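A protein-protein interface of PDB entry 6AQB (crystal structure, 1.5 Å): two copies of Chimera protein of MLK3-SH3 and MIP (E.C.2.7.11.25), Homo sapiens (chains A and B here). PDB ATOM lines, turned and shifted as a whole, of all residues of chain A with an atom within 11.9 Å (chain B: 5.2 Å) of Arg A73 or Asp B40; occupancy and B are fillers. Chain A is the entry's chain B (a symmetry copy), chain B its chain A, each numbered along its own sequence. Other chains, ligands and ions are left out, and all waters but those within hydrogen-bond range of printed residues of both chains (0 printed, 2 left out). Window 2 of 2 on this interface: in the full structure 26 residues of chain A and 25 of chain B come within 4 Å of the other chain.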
ATOM      1  N   ILE A  69     -16.625   4.525 -11.142  1.00  0.00           N
ATOM      2  CA  ILE A  69     -15.338   5.147 -10.966  1.00  0.00           C
ATOM      3  C   ILE A  69     -15.544   6.316 -10.034  1.00  0.00           C
ATOM      4  O   ILE A  69     -16.376   7.151 -10.291  1.00  0.00           O
ATOM      5  CB  ILE A  69     -14.763   5.608 -12.333  1.00  0.00           C
ATOM      6  CG1 ILE A  69     -14.459   4.391 -13.180  1.00  0.00           C
ATOM      7  CG2 ILE A  69     -13.471   6.428 -12.089  1.00  0.00           C
ATOM      8  CD1 ILE A  69     -14.180   4.587 -14.669  1.00  0.00           C
ATOM      9  N   PRO A  70     -14.738   6.425  -8.962  1.00  0.00           N
ATOM     10  CA  PRO A  70     -15.000   7.563  -8.119  1.00  0.00           C
ATOM     11  C   PRO A  70     -14.496   8.908  -8.737  1.00  0.00           C
ATOM     12  O   PRO A  70     -13.579   8.897  -9.608  1.00  0.00           O
ATOM     13  CB  PRO A  70     -14.221   7.284  -6.827  1.00  0.00           C
ATOM     14  CG  PRO A  70     -13.757   5.877  -6.931  1.00  0.00           C
ATOM     15  CD  PRO A  70     -13.701   5.549  -8.418  1.00  0.00           C
ATOM     16  N   PRO A  71     -15.058  10.001  -8.278  1.00  0.00           N
ATOM     17  CA  PRO A  71     -14.575  11.281  -8.803  1.00  0.00           C
ATOM     18  C   PRO A  71     -13.142  11.547  -8.434  1.00  0.00           C
ATOM     19  O   PRO A  71     -12.626  11.002  -7.459  1.00  0.00           O
ATOM     20  CB  PRO A  71     -15.490  12.307  -8.139  1.00  0.00           C
ATOM     21  CG  PRO A  71     -16.709  11.566  -7.749  1.00  0.00           C
ATOM     22  CD  PRO A  71     -16.206  10.190  -7.383  1.00  0.00           C
ATOM     23  N   PRO A  72     -12.453  12.405  -9.196  1.00  0.00           N
ATOM     24  CA  PRO A  72     -11.137  12.716  -8.759  1.00  0.00           C
ATOM     25  C   PRO A  72     -11.040  13.477  -7.410  1.00  0.00           C
ATOM     26  O   PRO A  72     -11.920  14.226  -7.094  1.00  0.00           O
ATOM     27  CB  PRO A  72     -10.592  13.634  -9.891  1.00  0.00           C
ATOM     28  CG  PRO A  72     -11.797  14.165 -10.552  1.00  0.00           C
ATOM     29  CD  PRO A  72     -12.834  13.064 -10.442  1.00  0.00           C
ATOM     30  N   ARG A  73      -9.917  13.313  -6.756  1.00  0.00           N
ATOM     31  CA  ARG A  73      -9.497  14.117  -5.610  1.00  0.00           C
ATOM     32  C   ARG A  73      -8.172  14.782  -5.945  1.00  0.00           C
ATOM     33  O   ARG A  73      -7.205  14.125  -6.376  1.00  0.00           O
ATOM     34  CB  ARG A  73      -9.286  13.283  -4.401  1.00  0.00           C
ATOM     35  CG  ARG A  73     -10.608  12.697  -3.875  1.00  0.00           C
ATOM     36  CD  ARG A  73     -10.343  12.069  -2.526  1.00  0.00           C
ATOM     37  NE  ARG A  73     -10.116  13.128  -1.557  1.00  0.00           N
ATOM     38  CZ  ARG A  73      -9.569  12.949  -0.356  1.00  0.00           C
ATOM     39  NH1 ARG A  73      -9.248  11.762   0.093  1.00  0.00           N
ATOM     40  NH2 ARG A  73      -9.371  14.013   0.427  1.00  0.00           N
ATOM     41  OXT ARG A  73      -8.102  15.987  -5.724  1.00  0.00           O
ATOM     42  N   GLY B  16      -7.478   6.996   1.198  1.00  0.00           N
ATOM     43  CA  GLY B  16      -6.980   8.248   1.769  1.00  0.00           C
ATOM     44  C   GLY B  16      -7.448   8.300   3.200  1.00  0.00           C
ATOM     45  O   GLY B  16      -8.510   7.752   3.529  1.00  0.00           O
ATOM     46  N   ASP B  18      -8.836  10.424   5.140  1.00  0.00           N
ATOM     47  CA  ASP B  18     -10.048  11.161   5.490  1.00  0.00           C
ATOM     48  C   ASP B  18     -11.264  10.501   4.820  1.00  0.00           C
ATOM     49  O   ASP B  18     -12.331  11.114   4.899  1.00  0.00           O
ATOM     50  CB  ASP B  18     -10.000  12.578   4.949  1.00  0.00           C
ATOM     51  CG  ASP B  18      -9.444  12.648   3.507  1.00  0.00           C
ATOM     52  OD1 ASP B  18      -8.980  11.571   2.933  1.00  0.00           O
ATOM     53  OD2 ASP B  18      -9.431  13.810   2.983  1.00  0.00           O
ATOM     54  N   GLU B  19     -11.095   9.360   4.160  1.00  0.00           N
ATOM     55  CA  GLU B  19     -12.173   8.694   3.432  1.00  0.00           C
ATOM     56  C   GLU B  19     -12.885   7.670   4.287  1.00  0.00           C
ATOM     57  O   GLU B  19     -12.259   6.889   5.002  1.00  0.00           O
ATOM     58  CB  GLU B  19     -11.646   7.956   2.206  1.00  0.00           C
ATOM     59  CG  GLU B  19     -10.984   8.959   1.239  1.00  0.00           C
ATOM     60  CD  GLU B  19     -10.541   8.363  -0.057  1.00  0.00           C
ATOM     61  OE1 GLU B  19     -10.726   7.127  -0.284  1.00  0.00           O
ATOM     62  OE2 GLU B  19     -10.001   9.155  -0.909  1.00  0.00           O
ATOM     63  N   ALA B  35     -18.810  20.714  -1.640  1.00  0.00           N
ATOM     64  CA  ALA B  35     -17.391  20.448  -1.973  1.00  0.00           C
ATOM     65  C   ALA B  35     -16.381  21.294  -1.176  1.00  0.00           C
ATOM     66  O   ALA B  35     -15.209  20.909  -0.937  1.00  0.00           O
ATOM     67  CB  ALA B  35     -17.126  20.635  -3.472  1.00  0.00           C
ATOM     68  N   SER B  38     -16.147  18.894   1.780  1.00  0.00           N
ATOM     69  CA  SER B  38     -15.473  17.660   1.473  1.00  0.00           C
ATOM     70  C   SER B  38     -14.129  17.871   0.884  1.00  0.00           C
ATOM     71  O   SER B  38     -13.227  17.051   1.071  1.00  0.00           O
ATOM     72  CB  SER B  38     -16.285  16.810   0.498  1.00  0.00           C
ATOM     73  OG  SER B  38     -16.382  17.380  -0.770  1.00  0.00           O
ATOM     74  N   GLY B  39     -13.974  19.002   0.187  1.00  0.00           N
ATOM     75  CA  GLY B  39     -12.734  19.309  -0.421  1.00  0.00           C
ATOM     76  C   GLY B  39     -12.612  18.854  -1.843  1.00  0.00           C
ATOM     77  O   GLY B  39     -11.550  19.066  -2.444  1.00  0.00           O
ATOM     78  N   ASP B  40     -13.651  18.219  -2.400  1.00  0.00           N
ATOM     79  CA  ASP B  40     -13.619  17.772  -3.831  1.00  0.00           C
ATOM     80  C   ASP B  40     -15.019  17.602  -4.353  1.00  0.00           C
ATOM     81  O   ASP B  40     -15.891  17.051  -3.673  1.00  0.00           O
ATOM     82  CB  ASP B  40     -12.885  16.428  -3.931  1.00  0.00           C
ATOM     83  CG  ASP B  40     -11.361  16.533  -3.816  1.00  0.00           C
ATOM     84  OD1 ASP B  40     -10.708  16.996  -4.768  1.00  0.00           O
ATOM     85  OD2 ASP B  40     -10.761  16.087  -2.831  1.00  0.00           O
ATOM     86  N   GLU B  41     -15.267  18.034  -5.581  1.00  0.00           N
ATOM     87  CA  GLU B  41     -16.556  17.881  -6.167  1.00  0.00           C
ATOM     88  C   GLU B  41     -16.809  16.357  -6.272  1.00  0.00           C
ATOM     89  O   GLU B  41     -15.906  15.625  -6.531  1.00  0.00           O
ATOM     90  CB  GLU B  41     -16.612  18.541  -7.572  1.00  0.00           C
ATOM     91  CG  GLU B  41     -17.956  18.404  -8.292  1.00  0.00           C
ATOM     92  CD  GLU B  41     -18.125  17.150  -9.180  1.00  0.00           C
ATOM     93  OE1 GLU B  41     -17.159  16.363  -9.377  1.00  0.00           O
ATOM     94  OE2 GLU B  41     -19.253  16.936  -9.704  1.00  0.00           O
ATOM     95  N   GLY B  42     -18.048  15.995  -6.038  1.00  0.00           N
ATOM     96  CA  GLY B  42     -18.532  14.634  -6.170  1.00  0.00           C
ATOM     97  C   GLY B  42     -18.182  13.839  -4.951  1.00  0.00           C
ATOM     98  O   GLY B  42     -18.528  12.666  -4.940  1.00  0.00           O
ATOM     99  N   TRP B  43     -17.515  14.439  -3.956  1.00  0.00           N
ATOM    100  CA  TRP B  43     -17.233  13.758  -2.627  1.00  0.00           C
ATOM    101  C   TRP B  43     -18.057  14.450  -1.570  1.00  0.00           C
ATOM    102  O   TRP B  43     -18.132  15.681  -1.540  1.00  0.00           O
ATOM    103  CB  TRP B  43     -15.812  13.725  -2.253  1.00  0.00           C
ATOM    104  CG  TRP B  43     -14.958  12.907  -3.103  1.00  0.00           C
ATOM    105  CD1 TRP B  43     -14.620  13.147  -4.398  1.00  0.00           C
ATOM    106  CD2 TRP B  43     -14.414  11.644  -2.775  1.00  0.00           C
ATOM    107  NE1 TRP B  43     -13.858  12.163  -4.869  1.00  0.00           N
ATOM    108  CE2 TRP B  43     -13.722  11.195  -3.912  1.00  0.00           C
ATOM    109  CE3 TRP B  43     -14.368  10.870  -1.604  1.00  0.00           C
ATOM    110  CZ2 TRP B  43     -13.031  10.011  -3.952  1.00  0.00           C
ATOM    111  CZ3 TRP B  43     -13.684   9.670  -1.659  1.00  0.00           C
ATOM    112  CH2 TRP B  43     -13.021   9.249  -2.806  1.00  0.00           C
ATOM    113  N   ILE B  54     -15.105  11.358   4.237  1.00  0.00           N
ATOM    114  CA  ILE B  54     -15.681  11.635   2.966  1.00  0.00           C
ATOM    115  C   ILE B  54     -15.800  10.404   2.122  1.00  0.00           C
ATOM    116  O   ILE B  54     -15.095   9.422   2.307  1.00  0.00           O
ATOM    117  CB  ILE B  54     -14.880  12.747   2.208  1.00  0.00           C
ATOM    118  CG1 ILE B  54     -13.466  12.362   1.973  1.00  0.00           C
ATOM    119  CG2 ILE B  54     -15.098  14.085   2.948  1.00  0.00           C
ATOM    120  CD1 ILE B  54     -12.737  13.298   1.029  1.00  0.00           C
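The guanidinium group of Arg A73 lies within salt-bridge range of the side-chain carboxylate of Asp B18 (2.6 Å).
OE2 of Glu B19 is in salt-bridge range of NH1 of Arg A73, at 2.9 Å.
OD2 of Asp B40 lies within salt-bridge range of NE of Arg A73, 3.3 Å away.
The backbone carbonyl oxygen (O) of Pro A71 sits at hydrogen-bond distance from the indole nitrogen (NE1) of Trp B43 (3.1 Å).
N of Ile B54 is in hydrogen-bond range of O of Asp B18 (2.9 Å).
The backbone NH (N) of Asp B40 lies within hydrogen-bond range of the backbone carbonyl oxygen (O) of Ala B35 (3.4 Å).
OG of Ser B38 is in hydrogen-bond range of O of Asp B40 (3.0 Å).
OG of Ser B38 sits at hydrogen-bond distance from O of Trp B43, at 2.6 Å.
Among the printed residues, merely in contact across the chains: Pro A71 with Glu B41 (3.7 Å), Pro A71 with Gly B42 (3.5 Å), Pro A72 with Asp B40 (3.8 Å), Pro A72 with Trp B43 (3.6 Å), Arg A73 with Trp B43 (3.4 Å) and Arg A73 with Ile B54 (3.5 Å).
Ile A69 touches none of the printed residues of chain B.
Printed residues of chain B within 4 Å of Pro A71: Glu B41, Gly B42 and Trp B43.
Of the printed residues of chain B, Pro A72 touches Asp B40 and Trp B43.
Of chain B, only Asp B18 (2.6 Å), Glu B19 (2.9 Å), Asp B40 (3.0 Å), Trp B43 (3.4 Å) and Ile B54 (3.5 Å) come within 4 Å of Arg A73.
No residue of chain A comes within 4 Å of Ser B38.
No residue of chain A comes within 4 Å of Gly B39.
Of chain A, only Pro A72 (3.8 Å) and Arg A73 (3.0 Å) come within 4 Å of Asp B40.
Of chain A, only Pro A71 (3.5 Å) comes within 4 Å of Gly B42.
Of chain A, only Pro A71, Pro A72 and Arg A73 come within 4 Å of Trp B43.
Ile B54 touches just one residue of chain A: Arg A73.
The nearest residue of chain B that does not touch Arg A73 is Gly B16 (4.5 Å).
The nearest residue of chain A that does not touch Asp B40 is Pro A71 (6.4 Å).
Of the 11 printed residues of chain B, 7 touch a printed residue of chain A.
Printed residues of chain B that touch a printed residue of chain A: Asp B18, Glu B19, Asp B40, Glu B41, Gly B42, Trp B43 and Ile B54.
Printed residues of chain A that touch a printed residue of chain B: Pro A71, Pro A72 and Arg A73.
Hydrophobic or aromatic side chains of chain A that line the printed part of chain B: Pro A71.
Among the printed residues, 10 pairs touch across the chains.
Among the printed residues, Asp or Glu carboxylates within 4 Å of a Lys or Arg side-chain nitrogen of the other chain: Arg A73 with Asp B18, Arg A73 with Glu B19 and Arg A73 with Asp B40.
No position is printed for both chains.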
